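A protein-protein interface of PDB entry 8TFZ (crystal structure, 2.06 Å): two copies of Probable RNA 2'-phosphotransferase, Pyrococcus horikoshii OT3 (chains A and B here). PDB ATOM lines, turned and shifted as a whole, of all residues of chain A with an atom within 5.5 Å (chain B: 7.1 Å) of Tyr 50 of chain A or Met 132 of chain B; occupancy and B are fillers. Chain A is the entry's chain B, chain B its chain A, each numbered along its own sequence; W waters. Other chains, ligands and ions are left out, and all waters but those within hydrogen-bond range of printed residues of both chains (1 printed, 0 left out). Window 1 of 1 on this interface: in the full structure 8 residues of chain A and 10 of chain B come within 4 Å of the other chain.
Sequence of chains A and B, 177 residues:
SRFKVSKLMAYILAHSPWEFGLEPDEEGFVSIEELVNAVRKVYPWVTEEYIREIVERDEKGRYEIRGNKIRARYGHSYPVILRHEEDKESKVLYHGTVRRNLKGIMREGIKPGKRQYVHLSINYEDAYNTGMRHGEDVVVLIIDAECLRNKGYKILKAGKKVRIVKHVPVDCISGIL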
ATOM      1  N   SER A   1      25.587 -12.705 -26.094  1.00  0.00           N
ATOM      2  CA  SER A   1      26.746 -11.985 -26.601  1.00  0.00           C
ATOM      3  C   SER A   1      26.686 -10.523 -26.186  1.00  0.00           C
ATOM      4  O   SER A   1      25.599  -9.995 -25.946  1.00  0.00           O
ATOM      5  CB  SER A   1      26.833 -12.108 -28.131  1.00  0.00           C
ATOM      6  OG  SER A   1      26.032 -11.131 -28.782  1.00  0.00           O
ATOM      7  N   ARG A   2      27.852  -9.872 -26.105  1.00  0.00           N
ATOM      8  CA  ARG A   2      27.889  -8.441 -25.810  1.00  0.00           C
ATOM      9  C   ARG A   2      27.038  -7.648 -26.803  1.00  0.00           C
ATOM     10  O   ARG A   2      26.450  -6.623 -26.451  1.00  0.00           O
ATOM     11  CB  ARG A   2      29.345  -7.964 -25.805  1.00  0.00           C
ATOM     12  CG  ARG A   2      29.585  -6.474 -25.600  1.00  0.00           C
ATOM     13  CD  ARG A   2      31.078  -6.158 -25.799  1.00  0.00           C
ATOM     14  NE  ARG A   2      31.361  -5.397 -27.015  1.00  0.00           N
ATOM     15  CZ  ARG A   2      32.494  -4.744 -27.251  1.00  0.00           C
ATOM     16  NH1 ARG A   2      33.487  -4.739 -26.371  1.00  0.00           N
ATOM     17  NH2 ARG A   2      32.645  -4.098 -28.407  1.00  0.00           N
ATOM     18  N   VAL A   5      23.270  -8.118 -25.725  1.00  0.00           N
ATOM     19  CA  VAL A   5      22.952  -7.442 -24.465  1.00  0.00           C
ATOM     20  C   VAL A   5      23.116  -5.931 -24.597  1.00  0.00           C
ATOM     21  O   VAL A   5      22.348  -5.165 -24.007  1.00  0.00           O
ATOM     22  CB  VAL A   5      23.777  -8.025 -23.303  1.00  0.00           C
ATOM     23  CG1 VAL A   5      25.168  -8.142 -23.717  1.00  0.00           C
ATOM     24  CG2 VAL A   5      23.667  -7.143 -22.048  1.00  0.00           C
ATOM     25  N   TRP A  45      22.068 -14.518 -17.292  1.00  0.00           N
ATOM     26  CA  TRP A  45      23.458 -14.519 -16.844  1.00  0.00           C
ATOM     27  C   TRP A  45      24.026 -13.125 -16.624  1.00  0.00           C
ATOM     28  O   TRP A  45      25.052 -12.991 -15.959  1.00  0.00           O
ATOM     29  CB  TRP A  45      24.356 -15.232 -17.856  1.00  0.00           C
ATOM     30  CG  TRP A  45      24.153 -14.740 -19.251  1.00  0.00           C
ATOM     31  CD1 TRP A  45      24.819 -13.708 -19.895  1.00  0.00           C
ATOM     32  CD2 TRP A  45      23.200 -15.247 -20.177  1.00  0.00           C
ATOM     33  NE1 TRP A  45      24.333 -13.573 -21.183  1.00  0.00           N
ATOM     34  CE2 TRP A  45      23.345 -14.513 -21.377  1.00  0.00           C
ATOM     35  CE3 TRP A  45      22.242 -16.273 -20.116  1.00  0.00           C
ATOM     36  CZ2 TRP A  45      22.564 -14.773 -22.496  1.00  0.00           C
ATOM     37  CZ3 TRP A  45      21.467 -16.529 -21.231  1.00  0.00           C
ATOM     38  CH2 TRP A  45      21.623 -15.768 -22.403  1.00  0.00           C
ATOM     39  N   VAL A  46      23.417 -12.089 -17.185  1.00  0.00           N
ATOM     40  CA  VAL A  46      24.007 -10.759 -17.125  1.00  0.00           C
ATOM     41  C   VAL A  46      24.162 -10.288 -15.680  1.00  0.00           C
ATOM     42  O   VAL A  46      23.256 -10.449 -14.849  1.00  0.00           O
ATOM     43  CB  VAL A  46      23.171  -9.784 -17.956  1.00  0.00           C
ATOM     44  CG1 VAL A  46      23.631  -8.360 -17.686  1.00  0.00           C
ATOM     45  CG2 VAL A  46      23.322 -10.140 -19.435  1.00  0.00           C
ATOM     46  N   THR A  47      25.342  -9.744 -15.365  1.00  0.00           N
ATOM     47  CA  THR A  47      25.625  -9.173 -14.061  1.00  0.00           C
ATOM     48  C   THR A  47      25.872  -7.682 -14.202  1.00  0.00           C
ATOM     49  O   THR A  47      25.997  -7.146 -15.303  1.00  0.00           O
ATOM     50  CB  THR A  47      26.848  -9.834 -13.409  1.00  0.00           C
ATOM     51  OG1 THR A  47      27.988  -9.712 -14.280  1.00  0.00           O
ATOM     52  CG2 THR A  47      26.572 -11.325 -13.106  1.00  0.00           C
ATOM     53  N   GLU A  48      25.944  -7.009 -13.060  1.00  0.00           N
ATOM     54  CA  GLU A  48      26.310  -5.604 -13.077  1.00  0.00           C
ATOM     55  C   GLU A  48      27.742  -5.406 -13.560  1.00  0.00           C
ATOM     56  O   GLU A  48      28.030  -4.425 -14.248  1.00  0.00           O
ATOM     57  CB  GLU A  48      26.098  -4.998 -11.693  1.00  0.00           C
ATOM     58  CG  GLU A  48      26.663  -3.614 -11.542  1.00  0.00           C
ATOM     59  CD  GLU A  48      26.215  -2.905 -10.270  1.00  0.00           C
ATOM     60  OE1 GLU A  48      25.283  -3.364  -9.580  1.00  0.00           O
ATOM     61  OE2 GLU A  48      26.821  -1.866  -9.961  1.00  0.00           O
ATOM     62  N   GLU A  49      28.652  -6.330 -13.239  1.00  0.00           N
ATOM     63  CA  GLU A  49      30.005  -6.221 -13.782  1.00  0.00           C
ATOM     64  C   GLU A  49      30.016  -6.333 -15.314  1.00  0.00           C
ATOM     65  O   GLU A  49      30.774  -5.623 -15.985  1.00  0.00           O
ATOM     66  CB  GLU A  49      30.906  -7.249 -13.083  1.00  0.00           C
ATOM     67  CG  GLU A  49      30.828  -8.691 -13.548  1.00  0.00           C
ATOM     68  CD  GLU A  49      31.651  -9.654 -12.671  1.00  0.00           C
ATOM     69  OE1 GLU A  49      32.877  -9.392 -12.432  1.00  0.00           O
ATOM     70  OE2 GLU A  49      31.092 -10.728 -12.281  1.00  0.00           O
ATOM     71  N   TYR A  50      29.135  -7.158 -15.887  1.00  0.00           N
ATOM     72  CA  TYR A  50      29.104  -7.305 -17.338  1.00  0.00           C
ATOM     73  C   TYR A  50      28.612  -6.027 -18.012  1.00  0.00           C
ATOM     74  O   TYR A  50      29.140  -5.613 -19.050  1.00  0.00           O
ATOM     75  CB  TYR A  50      28.225  -8.492 -17.712  1.00  0.00           C
ATOM     76  CG  TYR A  50      28.325  -8.949 -19.155  1.00  0.00           C
ATOM     77  CD1 TYR A  50      29.505  -9.489 -19.665  1.00  0.00           C
ATOM     78  CD2 TYR A  50      27.217  -8.885 -19.994  1.00  0.00           C
ATOM     79  CE1 TYR A  50      29.586  -9.934 -20.998  1.00  0.00           C
ATOM     80  CE2 TYR A  50      27.281  -9.325 -21.322  1.00  0.00           C
ATOM     81  CZ  TYR A  50      28.464  -9.840 -21.822  1.00  0.00           C
ATOM     82  OH  TYR A  50      28.498 -10.268 -23.134  1.00  0.00           O
ATOM     83  N   ILE A  51      27.627  -5.378 -17.405  1.00  0.00           N
ATOM     84  CA  ILE A  51      27.083  -4.118 -17.903  1.00  0.00           C
ATOM     85  C   ILE A  51      28.099  -2.991 -17.774  1.00  0.00           C
ATOM     86  O   ILE A  51      28.226  -2.153 -18.673  1.00  0.00           O
ATOM     87  CB  ILE A  51      25.787  -3.804 -17.149  1.00  0.00           C
ATOM     88  CG1 ILE A  51      24.736  -4.845 -17.541  1.00  0.00           C
ATOM     89  CG2 ILE A  51      25.258  -2.340 -17.435  1.00  0.00           C
ATOM     90  CD1 ILE A  51      23.394  -4.414 -17.181  1.00  0.00           C
ATOM     91  N   ARG A  52      28.830  -2.944 -16.652  1.00  0.00           N
ATOM     92  CA  ARG A  52      29.848  -1.912 -16.510  1.00  0.00           C
ATOM     93  C   ARG A  52      30.971  -2.120 -17.514  1.00  0.00           C
ATOM     94  O   ARG A  52      31.489  -1.146 -18.088  1.00  0.00           O
ATOM     95  CB  ARG A  52      30.377  -1.880 -15.084  1.00  0.00           C
ATOM     96  CG  ARG A  52      29.450  -1.180 -14.114  1.00  0.00           C
ATOM     97  CD  ARG A  52      29.872  -1.535 -12.719  1.00  0.00           C
ATOM     98  NE  ARG A  52      29.079  -0.892 -11.677  1.00  0.00           N
ATOM     99  CZ  ARG A  52      29.130   0.391 -11.325  1.00  0.00           C
ATOM    100  NH1 ARG A  52      29.888   1.268 -11.971  1.00  0.00           N
ATOM    101  NH2 ARG A  52      28.379   0.810 -10.309  1.00  0.00           N
ATOM    102  N   GLU A  53      31.308  -3.387 -17.795  1.00  0.00           N
ATOM    103  CA  GLU A  53      32.282  -3.679 -18.840  1.00  0.00           C
ATOM    104  C   GLU A  53      31.806  -3.210 -20.217  1.00  0.00           C
ATOM    105  O   GLU A  53      32.593  -2.660 -20.997  1.00  0.00           O
ATOM    106  CB  GLU A  53      32.594  -5.172 -18.871  1.00  0.00           C
ATOM    107  CG  GLU A  53      33.901  -5.494 -19.580  1.00  0.00           C
ATOM    108  CD  GLU A  53      35.142  -5.000 -18.825  1.00  0.00           C
ATOM    109  OE1 GLU A  53      35.271  -3.775 -18.607  1.00  0.00           O
ATOM    110  OE2 GLU A  53      35.988  -5.829 -18.449  1.00  0.00           O
ATOM    111  N   ILE A  54      30.536  -3.440 -20.545  1.00  0.00           N
ATOM    112  CA  ILE A  54      30.005  -2.968 -21.832  1.00  0.00           C
ATOM    113  C   ILE A  54      30.123  -1.450 -21.932  1.00  0.00           C
ATOM    114  O   ILE A  54      30.639  -0.911 -22.922  1.00  0.00           O
ATOM    115  CB  ILE A  54      28.545  -3.427 -22.012  1.00  0.00           C
ATOM    116  CG1 ILE A  54      28.446  -4.922 -22.320  1.00  0.00           C
ATOM    117  CG2 ILE A  54      27.787  -2.576 -23.058  1.00  0.00           C
ATOM    118  CD1 ILE A  54      26.982  -5.394 -22.193  1.00  0.00           C
ATOM    119  N   VAL A  55      29.636  -0.734 -20.905  1.00  0.00           N
ATOM    120  CA  VAL A  55      29.774   0.723 -20.882  1.00  0.00           C
ATOM    121  C   VAL A  55      31.220   1.131 -21.169  1.00  0.00           C
ATOM    122  O   VAL A  55      31.475   2.061 -21.948  1.00  0.00           O
ATOM    123  CB  VAL A  55      29.301   1.290 -19.535  1.00  0.00           C
ATOM    124  CG1 VAL A  55      29.616   2.809 -19.448  1.00  0.00           C
ATOM    125  CG2 VAL A  55      27.853   1.012 -19.325  1.00  0.00           C
ATOM    126  N   PHE B   3      34.119  -1.472  -9.446  1.00  0.00           N
ATOM    127  CA  PHE B   3      34.332  -2.468 -10.497  1.00  0.00           C
ATOM    128  C   PHE B   3      35.743  -2.377 -11.083  1.00  0.00           C
ATOM    129  O   PHE B   3      36.453  -3.386 -11.196  1.00  0.00           O
ATOM    130  CB  PHE B   3      33.269  -2.256 -11.565  1.00  0.00           C
ATOM    131  CG  PHE B   3      33.645  -2.702 -12.934  1.00  0.00           C
ATOM    132  CD1 PHE B   3      33.496  -4.024 -13.317  1.00  0.00           C
ATOM    133  CD2 PHE B   3      34.081  -1.784 -13.867  1.00  0.00           C
ATOM    134  CE1 PHE B   3      33.795  -4.447 -14.638  1.00  0.00           C
ATOM    135  CE2 PHE B   3      34.382  -2.167 -15.161  1.00  0.00           C
ATOM    136  CZ  PHE B   3      34.237  -3.512 -15.558  1.00  0.00           C
ATOM    137  N   GLY B  96      30.488 -24.236 -17.850  1.00  0.00           N
ATOM    138  CA  GLY B  96      30.167 -23.488 -19.060  1.00  0.00           C
ATOM    139  C   GLY B  96      31.382 -23.533 -19.973  1.00  0.00           C
ATOM    140  O   GLY B  96      32.515 -23.394 -19.504  1.00  0.00           O
ATOM    141  N   THR B  97      31.129 -23.770 -21.265  1.00  0.00           N
ATOM    142  CA  THR B  97      32.174 -23.848 -22.282  1.00  0.00           C
ATOM    143  C   THR B  97      31.552 -23.449 -23.619  1.00  0.00           C
ATOM    144  O   THR B  97      30.388 -23.073 -23.681  1.00  0.00           O
ATOM    145  CB  THR B  97      32.792 -25.259 -22.323  1.00  0.00           C
ATOM    146  OG1 THR B  97      33.995 -25.247 -23.099  1.00  0.00           O
ATOM    147  CG2 THR B  97      31.833 -26.276 -22.912  1.00  0.00           C
ATOM    148  N   VAL B  98      32.340 -23.503 -24.697  1.00  0.00           N
ATOM    149  CA  VAL B  98      31.809 -23.271 -26.015  1.00  0.00           C
ATOM    150  C   VAL B  98      31.666 -24.596 -26.749  1.00  0.00           C
ATOM    151  O   VAL B  98      32.325 -25.596 -26.428  1.00  0.00           O
ATOM    152  CB  VAL B  98      32.658 -22.283 -26.826  1.00  0.00           C
ATOM    153  CG1 VAL B  98      32.273 -20.926 -26.418  1.00  0.00           C
ATOM    154  CG2 VAL B  98      34.133 -22.558 -26.611  1.00  0.00           C
ATOM    155  N   ASP B 126      26.132 -18.548 -13.683  1.00  0.00           N
ATOM    156  CA  ASP B 126      27.563 -18.313 -13.540  1.00  0.00           C
ATOM    157  C   ASP B 126      28.370 -19.130 -14.529  1.00  0.00           C
ATOM    158  O   ASP B 126      29.321 -18.615 -15.123  1.00  0.00           O
ATOM    159  CB  ASP B 126      28.023 -18.640 -12.127  1.00  0.00           C
ATOM    160  CG  ASP B 126      27.766 -17.541 -11.193  1.00  0.00           C
ATOM    161  OD1 ASP B 126      26.597 -17.147 -11.068  1.00  0.00           O
ATOM    162  OD2 ASP B 126      28.751 -17.013 -10.628  1.00  0.00           O
ATOM    163  N   ALA B 127      28.040 -20.425 -14.691  1.00  0.00           N
ATOM    164  CA  ALA B 127      28.784 -21.214 -15.655  1.00  0.00           C
ATOM    165  C   ALA B 127      28.680 -20.610 -17.045  1.00  0.00           C
ATOM    166  O   ALA B 127      29.685 -20.544 -17.769  1.00  0.00           O
ATOM    167  CB  ALA B 127      28.341 -22.662 -15.652  1.00  0.00           C
ATOM    168  N   TYR B 128      27.497 -20.124 -17.422  1.00  0.00           N
ATOM    169  CA  TYR B 128      27.329 -19.501 -18.741  1.00  0.00           C
ATOM    170  C   TYR B 128      28.174 -18.238 -18.873  1.00  0.00           C
ATOM    171  O   TYR B 128      28.861 -18.031 -19.891  1.00  0.00           O
ATOM    172  CB  TYR B 128      25.854 -19.183 -18.978  1.00  0.00           C
ATOM    173  CG  TYR B 128      25.530 -18.659 -20.375  1.00  0.00           C
ATOM    174  CD1 TYR B 128      24.900 -19.474 -21.337  1.00  0.00           C
ATOM    175  CD2 TYR B 128      25.838 -17.343 -20.730  1.00  0.00           C
ATOM    176  CE1 TYR B 128      24.614 -18.988 -22.627  1.00  0.00           C
ATOM    177  CE2 TYR B 128      25.571 -16.857 -22.010  1.00  0.00           C
ATOM    178  CZ  TYR B 128      24.955 -17.678 -22.949  1.00  0.00           C
ATOM    179  OH  TYR B 128      24.690 -17.140 -24.211  1.00  0.00           O
ATOM    180  N   ASN B 129      28.096 -17.357 -17.867  1.00  0.00           N
ATOM    181  CA  ASN B 129      28.894 -16.137 -17.860  1.00  0.00           C
ATOM    182  C   ASN B 129      30.382 -16.437 -18.010  1.00  0.00           C
ATOM    183  O   ASN B 129      31.109 -15.691 -18.677  1.00  0.00           O
ATOM    184  CB  ASN B 129      28.652 -15.351 -16.569  1.00  0.00           C
ATOM    185  CG  ASN B 129      27.461 -14.461 -16.659  1.00  0.00           C
ATOM    186  OD1 ASN B 129      27.368 -13.607 -17.560  1.00  0.00           O
ATOM    187  ND2 ASN B 129      26.519 -14.619 -15.698  1.00  0.00           N
ATOM    188  N   THR B 130      30.856 -17.516 -17.387  1.00  0.00           N
ATOM    189  CA  THR B 130      32.274 -17.821 -17.490  1.00  0.00           C
ATOM    190  C   THR B 130      32.609 -18.503 -18.802  1.00  0.00           C
ATOM    191  O   THR B 130      33.701 -18.286 -19.338  1.00  0.00           O
ATOM    192  CB  THR B 130      32.726 -18.708 -16.338  1.00  0.00           C
ATOM    193  OG1 THR B 130      31.977 -19.917 -16.379  1.00  0.00           O
ATOM    194  CG2 THR B 130      32.502 -18.047 -14.999  1.00  0.00           C
ATOM    195  N   GLY B 131      31.692 -19.334 -19.318  1.00  0.00           N
ATOM    196  CA  GLY B 131      31.933 -20.020 -20.570  1.00  0.00           C
ATOM    197  C   GLY B 131      31.988 -19.073 -21.743  1.00  0.00           C
ATOM    198  O   GLY B 131      32.619 -19.383 -22.751  1.00  0.00           O
ATOM    199  N   MET B 132      31.317 -17.919 -21.616  1.00  0.00           N
ATOM    200  CA  MET B 132      31.340 -16.801 -22.557  1.00  0.00           C
ATOM    201  C   MET B 132      32.738 -16.201 -22.796  1.00  0.00           C
ATOM    202  O   MET B 132      32.939 -15.518 -23.808  1.00  0.00           O
ATOM    203  CB  MET B 132      30.436 -15.715 -21.992  1.00  0.00           C
ATOM    204  CG  MET B 132      29.447 -15.069 -22.878  1.00  0.00           C
ATOM    205  SD  MET B 132      28.303 -14.193 -21.734  1.00  0.00           S
ATOM    206  CE  MET B 132      29.483 -13.294 -20.726  1.00  0.00           C
ATOM    207  N   ARG B 133      33.684 -16.391 -21.884  1.00  0.00           N
ATOM    208  CA  ARG B 133      35.039 -15.893 -22.137  1.00  0.00           C
ATOM    209  C   ARG B 133      35.643 -16.477 -23.418  1.00  0.00           C
ATOM    210  O   ARG B 133      36.465 -15.831 -24.069  1.00  0.00           O
ATOM    211  CB  ARG B 133      35.931 -16.177 -20.924  1.00  0.00           C
ATOM    212  CG  ARG B 133      35.644 -15.216 -19.742  1.00  0.00           C
ATOM    213  CD  ARG B 133      36.157 -15.651 -18.344  1.00  0.00           C
ATOM    214  NE  ARG B 133      37.613 -15.740 -18.204  1.00  0.00           N
ATOM    215  CZ  ARG B 133      38.436 -14.707 -18.018  1.00  0.00           C
ATOM    216  NH1 ARG B 133      38.003 -13.446 -18.050  1.00  0.00           N
ATOM    217  NH2 ARG B 133      39.740 -14.933 -17.812  1.00  0.00           N
ATOM    218  N   HIS B 134      35.206 -17.656 -23.844  1.00  0.00           N
ATOM    219  CA  HIS B 134      35.833 -18.324 -24.978  1.00  0.00           C
ATOM    220  C   HIS B 134      35.050 -18.204 -26.267  1.00  0.00           C
ATOM    221  O   HIS B 134      35.455 -18.807 -27.275  1.00  0.00           O
ATOM    222  CB  HIS B 134      36.070 -19.789 -24.655  1.00  0.00           C
ATOM    223  CG  HIS B 134      36.977 -19.984 -23.501  1.00  0.00           C
ATOM    224  ND1 HIS B 134      38.346 -19.858 -23.616  1.00  0.00           N
ATOM    225  CD2 HIS B 134      36.723 -20.248 -22.195  1.00  0.00           C
ATOM    226  CE1 HIS B 134      38.896 -20.049 -22.430  1.00  0.00           C
ATOM    227  NE2 HIS B 134      37.935 -20.283 -21.550  1.00  0.00           N
ATOM    228  N   GLY B 135      33.970 -17.441 -26.279  1.00  0.00           N
ATOM    229  CA  GLY B 135      33.230 -17.243 -27.507  1.00  0.00           C
ATOM    230  C   GLY B 135      31.747 -17.132 -27.232  1.00  0.00           C
ATOM    231  O   GLY B 135      31.284 -17.303 -26.098  1.00  0.00           O
ATOM    232  N   GLU B 136      31.014 -16.883 -28.322  1.00  0.00           N
ATOM    233  CA  GLU B 136      29.570 -16.655 -28.316  1.00  0.00           C
ATOM    234  C   GLU B 136      28.747 -17.931 -28.157  1.00  0.00           C
ATOM    235  O   GLU B 136      27.642 -17.885 -27.601  1.00  0.00           O
ATOM    236  CB  GLU B 136      29.142 -15.993 -29.632  1.00  0.00           C
ATOM    237  CG  GLU B 136      29.480 -14.539 -29.763  1.00  0.00           C
ATOM    238  CD  GLU B 136      28.914 -13.929 -31.042  1.00  0.00           C
ATOM    239  OE1 GLU B 136      28.027 -14.585 -31.662  1.00  0.00           O
ATOM    240  OE2 GLU B 136      29.351 -12.821 -31.430  1.00  0.00           O
ATOM    241  N   ASP B 137      29.208 -19.049 -28.714  1.00  0.00           N
ATOM    242  CA  ASP B 137      28.383 -20.232 -28.853  1.00  0.00           C
ATOM    243  C   ASP B 137      28.554 -21.103 -27.612  1.00  0.00           C
ATOM    244  O   ASP B 137      29.149 -22.189 -27.635  1.00  0.00           O
ATOM    245  CB  ASP B 137      28.726 -20.980 -30.140  1.00  0.00           C
ATOM    246  CG  ASP B 137      27.685 -22.062 -30.466  1.00  0.00           C
ATOM    247  OD1 ASP B 137      26.603 -21.964 -29.868  1.00  0.00           O
ATOM    248  OD2 ASP B 137      27.927 -22.996 -31.285  1.00  0.00           O
ATOM    249  N   VAL B 138      28.008 -20.575 -26.508  1.00  0.00           N
ATOM    250  CA  VAL B 138      28.175 -21.148 -25.165  1.00  0.00           C
ATOM    251  C   VAL B 138      27.216 -22.316 -24.950  1.00  0.00           C
ATOM    252  O   VAL B 138      26.037 -22.219 -25.289  1.00  0.00           O
ATOM    253  CB  VAL B 138      27.944 -20.054 -24.110  1.00  0.00           C
ATOM    254  CG1 VAL B 138      27.895 -20.633 -22.743  1.00  0.00           C
ATOM    255  CG2 VAL B 138      29.062 -19.015 -24.228  1.00  0.00           C
HETATM  256  O   HOH W   1      31.296  -0.742  -9.431  1.00  0.00           O
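O of Trp 45 of chain A lies close to OD1 of Asn 129 of chain B, 2.9 Å away.
The side-chain hydroxyl (OH) of Tyr 50 of chain A is in hydrogen-bond range of the backbone NH (N) of Arg 2 of chain A (3.1 Å). The backbone NH of Tyr 50 of chain A is in hydrogen-bond range of the side-chain hydroxyl of Thr 47 of chain A. OE2 of Glu 48 of chain A lies within salt-bridge range of NE of Arg 52 of chain A (3.0 Å).
Among the printed residues, pairs that only touch across the chains: Glu 53 of chain A with Phe 3 of chain B (3.2 Å), Trp 45 of chain A with Tyr 128 of chain B (3.3 Å), Tyr 50 of chain A with Met 132 of chain B (3.4 Å), Glu 49 of chain A with Phe 3 of chain B (3.5 Å), Arg 52 of chain A with Phe 3 of chain B (3.7 Å), Ser 1 of chain A with Glu 136 of chain B (3.9 Å) and Trp 45 of chain A with Met 132 of chain B (3.97 Å).
Printed residues of chain B within 4 Å of Ser 1 of chain A: Glu 136 (3.9 Å). Printed residues of chain B within 4 Å of Trp 45 of chain A: Tyr 128 (3.3 Å), Asn 129 (2.2 Å) and Met 132 (3.97 Å). Of chain B, only Met 132 (3.4 Å) comes within 4 Å of Tyr 50 of chain A. Printed residues of chain B within 4 Å of Glu 53 of chain A: Phe 3 (3.2 Å). Met 132 of chain B touches two residues of chain A. His 134 of chain B touches none of the printed residues of chain A. The nearest printed residue of chain A that does not touch Glu 136 of chain B is Arg 2 of chain A (6.1 Å).
Hydrophobic or aromatic side chains of chain B that line the printed part of chain A: Phe 3, Tyr 128 and Met 132. Among the printed residues, 8 pairs touch across the chains.
No position is printed for both chains. Of the 8 pairs that touch across the chains among the printed residues, none has its exchanged pair printed and touching as well.
Water W1 bridges N of Phe 3 of chain B and NE of Arg 52 of chain A.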
